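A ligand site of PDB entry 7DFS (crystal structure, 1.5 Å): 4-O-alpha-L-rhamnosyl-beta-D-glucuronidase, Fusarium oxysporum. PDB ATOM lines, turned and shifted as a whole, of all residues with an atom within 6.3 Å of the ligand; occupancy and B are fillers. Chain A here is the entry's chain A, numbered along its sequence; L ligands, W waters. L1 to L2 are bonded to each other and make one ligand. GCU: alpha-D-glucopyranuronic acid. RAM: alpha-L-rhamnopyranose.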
ATOM      1  N   SER A 279      20.579   5.992   5.224  1.00  0.00           N
ATOM      2  CA  SER A 279      20.845   6.840   4.024  1.00  0.00           C
ATOM      3  C   SER A 279      20.776   6.047   2.716  1.00  0.00           C
ATOM      4  O   SER A 279      20.391   6.605   1.692  1.00  0.00           O
ATOM      5  CB  SER A 279      22.116   7.585   4.141  1.00  0.00           C
ATOM      6  OG  SER A 279      22.037   8.543   5.189  1.00  0.00           O
ATOM      7  N   PRO A 280      21.125   4.732   2.635  1.00  0.00           N
ATOM      8  CA  PRO A 280      21.089   4.010   1.352  1.00  0.00           C
ATOM      9  C   PRO A 280      19.703   3.477   1.017  1.00  0.00           C
ATOM     10  O   PRO A 280      19.528   2.739   0.063  1.00  0.00           O
ATOM     11  CB  PRO A 280      22.063   2.828   1.542  1.00  0.00           C
ATOM     12  CG  PRO A 280      22.794   3.141   2.795  1.00  0.00           C
ATOM     13  CD  PRO A 280      21.886   3.990   3.665  1.00  0.00           C
ATOM     14  N   ILE A 310      34.530   8.036  -2.093  1.00  0.00           N
ATOM     15  CA  ILE A 310      34.187   6.882  -2.943  1.00  0.00           C
ATOM     16  C   ILE A 310      34.519   5.594  -2.184  1.00  0.00           C
ATOM     17  O   ILE A 310      35.657   5.463  -1.713  1.00  0.00           O
ATOM     18  CB  ILE A 310      34.902   6.976  -4.293  1.00  0.00           C
ATOM     19  CG1 ILE A 310      34.509   8.271  -5.013  1.00  0.00           C
ATOM     20  CG2 ILE A 310      34.629   5.774  -5.152  1.00  0.00           C
ATOM     21  CD1 ILE A 310      35.511   8.712  -6.080  1.00  0.00           C
ATOM     22  N   GLY A 311      33.505   4.753  -2.034  1.00  0.00           N
ATOM     23  CA  GLY A 311      33.619   3.495  -1.259  1.00  0.00           C
ATOM     24  C   GLY A 311      33.328   3.693   0.212  1.00  0.00           C
ATOM     25  O   GLY A 311      33.470   2.720   0.960  1.00  0.00           O
ATOM     26  N   ASN A 312      33.036   4.918   0.675  1.00  0.00           N
ATOM     27  CA  ASN A 312      32.637   5.136   2.092  1.00  0.00           C
ATOM     28  C   ASN A 312      31.588   6.264   2.127  1.00  0.00           C
ATOM     29  O   ASN A 312      31.809   7.284   2.747  1.00  0.00           O
ATOM     30  CB  ASN A 312      33.847   5.389   2.971  1.00  0.00           C
ATOM     31  CG  ASN A 312      33.521   5.421   4.450  1.00  0.00           C
ATOM     32  OD1 ASN A 312      32.434   4.977   4.862  1.00  0.00           O
ATOM     33  ND2 ASN A 312      34.437   5.894   5.260  1.00  0.00           N
ATOM     34  N   CYS A 313      30.472   6.018   1.488  1.00  0.00           N
ATOM     35  CA  CYS A 313      29.426   7.040   1.298  1.00  0.00           C
ATOM     36  C   CYS A 313      28.038   6.406   1.321  1.00  0.00           C
ATOM     37  O   CYS A 313      27.701   5.630   0.398  1.00  0.00           O
ATOM     38  CB  CYS A 313      29.655   7.721  -0.036  1.00  0.00           C
ATOM     39  SG  CYS A 313      28.391   8.995  -0.302  1.00  0.00           S
ATOM     40  N   GLN A 314      27.295   6.628   2.411  1.00  0.00           N
ATOM     41  CA  GLN A 314      25.995   5.969   2.581  1.00  0.00           C
ATOM     42  C   GLN A 314      24.883   6.697   1.823  1.00  0.00           C
ATOM     43  O   GLN A 314      23.901   6.058   1.517  1.00  0.00           O
ATOM     44  CB  GLN A 314      25.648   5.940   4.067  1.00  0.00           C
ATOM     45  CG  GLN A 314      26.642   5.165   4.923  1.00  0.00           C
ATOM     46  CD  GLN A 314      27.172   3.873   4.351  1.00  0.00           C
ATOM     47  OE1 GLN A 314      26.480   2.871   4.179  1.00  0.00           O
ATOM     48  NE2 GLN A 314      28.462   3.889   4.055  1.00  0.00           N
ATOM     49  N   TYR A 315      25.011   8.004   1.519  1.00  0.00           N
ATOM     50  CA  TYR A 315      23.923   8.776   0.880  1.00  0.00           C
ATOM     51  C   TYR A 315      24.166   8.961  -0.611  1.00  0.00           C
ATOM     52  O   TYR A 315      23.315   9.561  -1.271  1.00  0.00           O
ATOM     53  CB  TYR A 315      23.692  10.115   1.569  1.00  0.00           C
ATOM     54  CG  TYR A 315      24.867  10.962   1.918  1.00  0.00           C
ATOM     55  CD1 TYR A 315      25.824  11.303   0.963  1.00  0.00           C
ATOM     56  CD2 TYR A 315      25.036  11.468   3.194  1.00  0.00           C
ATOM     57  CE1 TYR A 315      26.911  12.077   1.268  1.00  0.00           C
ATOM     58  CE2 TYR A 315      26.107  12.288   3.514  1.00  0.00           C
ATOM     59  CZ  TYR A 315      27.049  12.594   2.542  1.00  0.00           C
ATOM     60  OH  TYR A 315      28.150  13.326   2.808  1.00  0.00           O
ATOM     61  N   CYS A 316      25.220   8.374  -1.146  1.00  0.00           N
ATOM     62  CA  CYS A 316      25.554   8.445  -2.593  1.00  0.00           C
ATOM     63  C   CYS A 316      24.513   7.734  -3.441  1.00  0.00           C
ATOM     64  O   CYS A 316      23.998   6.686  -3.095  1.00  0.00           O
ATOM     65  CB  CYS A 316      26.931   7.867  -2.879  1.00  0.00           C
ATOM     66  SG  CYS A 316      28.249   8.988  -2.440  1.00  0.00           S
ATOM     67  N   TRP A 317      24.208   8.286  -4.610  1.00  0.00           N
ATOM     68  CA  TRP A 317      23.258   7.693  -5.564  1.00  0.00           C
ATOM     69  C   TRP A 317      23.877   6.492  -6.286  1.00  0.00           C
ATOM     70  O   TRP A 317      23.131   5.659  -6.829  1.00  0.00           O
ATOM     71  CB  TRP A 317      22.772   8.745  -6.539  1.00  0.00           C
ATOM     72  CG  TRP A 317      22.079   9.904  -5.903  1.00  0.00           C
ATOM     73  CD1 TRP A 317      21.647  10.006  -4.616  1.00  0.00           C
ATOM     74  CD2 TRP A 317      21.661  11.119  -6.564  1.00  0.00           C
ATOM     75  NE1 TRP A 317      21.053  11.240  -4.410  1.00  0.00           N
ATOM     76  CE2 TRP A 317      21.059  11.946  -5.590  1.00  0.00           C
ATOM     77  CE3 TRP A 317      21.839  11.604  -7.848  1.00  0.00           C
ATOM     78  CZ2 TRP A 317      20.602  13.235  -5.915  1.00  0.00           C
ATOM     79  CZ3 TRP A 317      21.398  12.870  -8.158  1.00  0.00           C
ATOM     80  CH2 TRP A 317      20.799  13.669  -7.190  1.00  0.00           C
ATOM     81  N   TRP A 318      25.200   6.509  -6.388  1.00  0.00           N
ATOM     82  CA  TRP A 318      25.947   5.417  -7.036  1.00  0.00           C
ATOM     83  C   TRP A 318      27.335   5.370  -6.406  1.00  0.00           C
ATOM     84  O   TRP A 318      27.819   6.374  -5.856  1.00  0.00           O
ATOM     85  CB  TRP A 318      26.036   5.597  -8.553  1.00  0.00           C
ATOM     86  CG  TRP A 318      26.869   6.780  -8.994  1.00  0.00           C
ATOM     87  CD1 TRP A 318      28.219   6.836  -9.165  1.00  0.00           C
ATOM     88  CD2 TRP A 318      26.385   8.113  -9.228  1.00  0.00           C
ATOM     89  NE1 TRP A 318      28.605   8.097  -9.526  1.00  0.00           N
ATOM     90  CE2 TRP A 318      27.504   8.902  -9.568  1.00  0.00           C
ATOM     91  CE3 TRP A 318      25.117   8.698  -9.243  1.00  0.00           C
ATOM     92  CZ2 TRP A 318      27.400  10.260  -9.891  1.00  0.00           C
ATOM     93  CZ3 TRP A 318      25.000  10.030  -9.557  1.00  0.00           C
ATOM     94  CH2 TRP A 318      26.130  10.794  -9.874  1.00  0.00           C
ATOM     95  N   GLY A 319      27.993   4.230  -6.611  1.00  0.00           N
ATOM     96  CA  GLY A 319      29.418   4.065  -6.354  1.00  0.00           C
ATOM     97  C   GLY A 319      30.108   3.388  -7.520  1.00  0.00           C
ATOM     98  O   GLY A 319      29.532   3.308  -8.616  1.00  0.00           O
ATOM     99  N   LYS A 320      31.331   2.947  -7.305  1.00  0.00           N
ATOM    100  CA  LYS A 320      32.106   2.218  -8.345  1.00  0.00           C
ATOM    101  C   LYS A 320      31.372   0.935  -8.730  1.00  0.00           C
ATOM    102  O   LYS A 320      31.396   0.530  -9.933  1.00  0.00           O
ATOM    103  CB  LYS A 320      33.499   1.904  -7.794  1.00  0.00           C
ATOM    104  CG  LYS A 320      34.577   1.722  -8.818  1.00  0.00           C
ATOM    105  CD  LYS A 320      35.964   1.624  -8.155  1.00  0.00           C
ATOM    106  CE  LYS A 320      36.458   2.943  -7.612  1.00  0.00           C
ATOM    107  NZ  LYS A 320      37.893   2.880  -7.241  1.00  0.00           N
ATOM    108  N   TYR A 321      30.745   0.280  -7.758  1.00  0.00           N
ATOM    109  CA  TYR A 321      30.272  -1.126  -7.927  1.00  0.00           C
ATOM    110  C   TYR A 321      28.764  -1.224  -7.853  1.00  0.00           C
ATOM    111  O   TYR A 321      28.217  -2.127  -8.480  1.00  0.00           O
ATOM    112  CB  TYR A 321      30.903  -2.095  -6.922  1.00  0.00           C
ATOM    113  CG  TYR A 321      32.406  -2.038  -6.973  1.00  0.00           C
ATOM    114  CD1 TYR A 321      33.080  -2.432  -8.110  1.00  0.00           C
ATOM    115  CD2 TYR A 321      33.129  -1.542  -5.911  1.00  0.00           C
ATOM    116  CE1 TYR A 321      34.465  -2.346  -8.195  1.00  0.00           C
ATOM    117  CE2 TYR A 321      34.512  -1.398  -5.994  1.00  0.00           C
ATOM    118  CZ  TYR A 321      35.174  -1.832  -7.125  1.00  0.00           C
ATOM    119  OH  TYR A 321      36.540  -1.734  -7.205  1.00  0.00           O
ATOM    120  N   SER A 322      28.068  -0.401  -7.061  1.00  0.00           N
ATOM    121  CA  SER A 322      26.606  -0.542  -6.892  1.00  0.00           C
ATOM    122  C   SER A 322      25.901   0.786  -7.119  1.00  0.00           C
ATOM    123  O   SER A 322      26.468   1.840  -6.839  1.00  0.00           O
ATOM    124  CB  SER A 322      26.296  -1.061  -5.513  1.00  0.00           C
ATOM    125  OG  SER A 322      24.914  -1.300  -5.314  1.00  0.00           O
ATOM    126  N   MET A 323      24.667   0.677  -7.530  1.00  0.00           N
ATOM    127  CA  MET A 323      23.698   1.790  -7.478  1.00  0.00           C
ATOM    128  C   MET A 323      23.162   1.917  -6.044  1.00  0.00           C
ATOM    129  O   MET A 323      23.288   0.948  -5.221  1.00  0.00           O
ATOM    130  CB  MET A 323      22.562   1.548  -8.478  1.00  0.00           C
ATOM    131  CG  MET A 323      23.034   1.646  -9.913  1.00  0.00           C
ATOM    132  SD  MET A 323      23.651   3.287 -10.376  1.00  0.00           S
ATOM    133  CE  MET A 323      22.223   4.304  -9.957  1.00  0.00           C
ATOM    134  N   GLY A 324      22.639   3.098  -5.718  1.00  0.00           N
ATOM    135  CA  GLY A 324      21.960   3.341  -4.437  1.00  0.00           C
ATOM    136  C   GLY A 324      20.491   3.625  -4.628  1.00  0.00           C
ATOM    137  O   GLY A 324      20.124   4.372  -5.570  1.00  0.00           O
ATOM    138  N   SER A 325      19.626   3.089  -3.768  1.00  0.00           N
ATOM    139  CA  SER A 325      18.180   3.373  -3.795  1.00  0.00           C
ATOM    140  C   SER A 325      17.919   4.872  -3.934  1.00  0.00           C
ATOM    141  O   SER A 325      16.945   5.217  -4.587  1.00  0.00           O
ATOM    142  CB  SER A 325      17.489   2.848  -2.602  1.00  0.00           C
ATOM    143  OG  SER A 325      17.500   1.400  -2.610  1.00  0.00           O
ATOM    144  N   PRO A 326      18.643   5.788  -3.276  1.00  0.00           N
ATOM    145  CA  PRO A 326      18.251   7.194  -3.382  1.00  0.00           C
ATOM    146  C   PRO A 326      18.281   7.749  -4.811  1.00  0.00           C
ATOM    147  O   PRO A 326      17.562   8.714  -5.082  1.00  0.00           O
ATOM    148  CB  PRO A 326      19.228   7.910  -2.451  1.00  0.00           C
ATOM    149  CG  PRO A 326      19.609   6.875  -1.401  1.00  0.00           C
ATOM    150  CD  PRO A 326      19.666   5.595  -2.229  1.00  0.00           C
ATOM    151  N   ARG A 408      17.234  -1.719   0.022  1.00  0.00           N
ATOM    152  CA  ARG A 408      18.517  -1.296  -0.499  1.00  0.00           C
ATOM    153  C   ARG A 408      18.887  -2.069  -1.772  1.00  0.00           C
ATOM    154  O   ARG A 408      18.747  -3.248  -1.828  1.00  0.00           O
ATOM    155  CB  ARG A 408      19.625  -1.483   0.526  1.00  0.00           C
ATOM    156  CG  ARG A 408      19.505  -0.580   1.723  1.00  0.00           C
ATOM    157  CD  ARG A 408      20.499  -0.966   2.810  1.00  0.00           C
ATOM    158  NE  ARG A 408      21.864  -0.898   2.335  1.00  0.00           N
ATOM    159  CZ  ARG A 408      22.882  -0.527   3.093  1.00  0.00           C
ATOM    160  NH1 ARG A 408      22.689  -0.180   4.341  1.00  0.00           N
ATOM    161  NH2 ARG A 408      24.095  -0.517   2.602  1.00  0.00           N
ATOM    162  N   ASP A 410      21.911  -2.495  -2.871  1.00  0.00           N
ATOM    163  CA  ASP A 410      23.079  -3.306  -2.537  1.00  0.00           C
ATOM    164  C   ASP A 410      22.783  -4.568  -1.753  1.00  0.00           C
ATOM    165  O   ASP A 410      23.653  -5.386  -1.595  1.00  0.00           O
ATOM    166  CB  ASP A 410      24.222  -2.525  -1.908  1.00  0.00           C
ATOM    167  CG  ASP A 410      23.884  -1.925  -0.592  1.00  0.00           C
ATOM    168  OD1 ASP A 410      22.767  -2.068  -0.141  1.00  0.00           O
ATOM    169  OD2 ASP A 410      24.763  -1.314  -0.022  1.00  0.00           O
HETATM  170  C1  GCU L   1      29.575  -3.016  -2.814  1.00  0.00           C
HETATM  171  C2  GCU L   1      28.761  -2.701  -1.610  1.00  0.00           C
HETATM  172  C3  GCU L   1      27.829  -1.496  -1.818  1.00  0.00           C
HETATM  173  C4  GCU L   1      28.631  -0.330  -2.409  1.00  0.00           C
HETATM  174  C5  GCU L   1      29.410  -0.790  -3.635  1.00  0.00           C
HETATM  175  C6  GCU L   1      30.226   0.364  -4.162  1.00  0.00           C
HETATM  176  O1  GCU L   1      28.694  -3.467  -3.822  1.00  0.00           O
HETATM  177  O2  GCU L   1      27.940  -3.819  -1.193  1.00  0.00           O
HETATM  178  O3  GCU L   1      27.294  -1.107  -0.537  1.00  0.00           O
HETATM  179  O4  GCU L   1      27.706   0.772  -2.792  1.00  0.00           O
HETATM  180  O5  GCU L   1      30.311  -1.883  -3.239  1.00  0.00           O
HETATM  181  O6A GCU L   1      29.815   0.918  -5.213  1.00  0.00           O
HETATM  182  O6B GCU L   1      31.274   0.778  -3.563  1.00  0.00           O
HETATM  183  C1  RAM L   2      28.122   2.006  -2.267  1.00  0.00           C
HETATM  184  C2  RAM L   2      27.453   2.973  -3.246  1.00  0.00           C
HETATM  185  C3  RAM L   2      25.946   3.016  -3.042  1.00  0.00           C
HETATM  186  C4  RAM L   2      25.558   3.135  -1.599  1.00  0.00           C
HETATM  187  C5  RAM L   2      26.351   2.138  -0.758  1.00  0.00           C
HETATM  188  C6  RAM L   2      26.079   2.280   0.709  1.00  0.00           C
HETATM  189  O2  RAM L   2      28.032   4.237  -3.034  1.00  0.00           O
HETATM  190  O3  RAM L   2      25.323   4.059  -3.872  1.00  0.00           O
HETATM  191  O4  RAM L   2      24.148   2.944  -1.438  1.00  0.00           O
HETATM  192  O5  RAM L   2      27.754   2.269  -0.950  1.00  0.00           O
HETATM  193  O   HOH W   1      32.303   2.930  -4.650  1.00  0.00           O
HETATM  194  O   HOH W   2      28.666  -0.505   1.750  1.00  0.00           O
HETATM  195  O   HOH W   3      23.033   5.301  -1.013  1.00  0.00           O
HETATM  196  O   HOH W   4      30.680  -5.139  -4.679  1.00  0.00           O
HETATM  197  O   HOH W   5      26.314  -5.292  -3.038  1.00  0.00           O
HETATM  198  O   HOH W   6      30.928   4.925  -3.130  1.00  0.00           O
HETATM  199  O   HOH W   7      32.740  -0.447  -1.666  1.00  0.00           O
HETATM  200  O   HOH W   8      32.324  -3.189  -0.841  1.00  0.00           O
HETATM  201  O   HOH W   9      30.079   3.637  -0.083  1.00  0.00           O
HETATM  202  O   HOH W  10      23.197   0.528  -2.492  1.00  0.00           O
HETATM  203  O   HOH W  11      26.351  -3.982   1.649  1.00  0.00           O
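The backbone NH (N) of Gly 324 sits at hydrogen-bond distance from the backbone carbonyl oxygen (O) of Trp 317 (2.8 Å). The guanidinium group (NH2) of Arg 408 lies within salt-bridge range of the side-chain carboxylate (OD2) of Asp 410, 2.8 Å away. SG of Cys 316 is disulfide-bonded to SG of Cys 313.
CB of Pro 280 touches O4 of RAM L2 (3.6 Å). O of Cys 313 touches O5 of RAM L2, 3.6 Å away. OE1 of Gln 314 touches C6 of RAM L2, 3.5 Å away. C of Trp 317 touches O3 of RAM L2, at 3.7 Å. C of Trp 318 touches O3 of RAM L2 (3.5 Å). CA of Gly 319 touches O6A of GCU L1, 3.4 Å away. C of Met 323 touches O3 of RAM L2 (3.7 Å). NH2 of Arg 408 touches C6 of RAM L2, at 3.9 Å. Hydrophobic or aromatic side chains that line the ligand: Pro 280 and Tyr 321. Within 4 Å of the ligand: Pro 280, Cys 313, Gln 314, Cys 316, Trp 317, Trp 318, Gly 319, Lys 320, Tyr 321, Ser 322, Met 323, Gly 324, Arg 408 and Asp 410. Along chain A the residues within 4 Å of the ligand span positions 280 to 410. The nearest printed residue that does not touch the ligand is Gly 311 (4.3 Å).
Water W1 lies within hydrogen-bond range of an oxygen (O6B) of GCU L1, the backbone NH (N) of Lys 320 and the backbone NH (N) of Gly 311. Water W3 lies within hydrogen-bond range of an oxygen (O4) of RAM L2 (2.6 Å), the backbone carbonyl oxygen (O) of Cys 316 (2.7 Å) and the backbone carbonyl oxygen (O) of Gln 314 (2.8 Å). Water W10 lies within hydrogen-bond range of O of Met 323, O4 of RAM L2 and N of Asp 410. Water W9 lies within hydrogen-bond range of O5 of RAM L2 (2.8 Å), N of Cys 313 (2.9 Å) and N of Asn 312 (3.3 Å). Water W5 bridges an oxygen (O2) of GCU L1 (2.9 Å) and the backbone carbonyl oxygen (O) of Asp 410 (3.0 Å). Water W6 bridges N of Gly 311 and O2 of RAM L2.
O3 of RAM L2 lies within hydrogen-bond range of N of Gly 324, at 3.4 Å. The side-chain carboxylate (OD2) of Asp 410 is in hydrogen-bond range of an oxygen (O3) of GCU L1 (2.6 Å). N of Tyr 321 is in hydrogen-bond range of O6A of GCU L1 (2.8 Å). An oxygen (O6A) of GCU L1 is in hydrogen-bond range of the backbone NH of Lys 320. O of Cys 316 lies within hydrogen-bond range of O3 of RAM L2 (3.0 Å). O6A of GCU L1 sits at hydrogen-bond distance from N of Ser 322 (2.9 Å).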
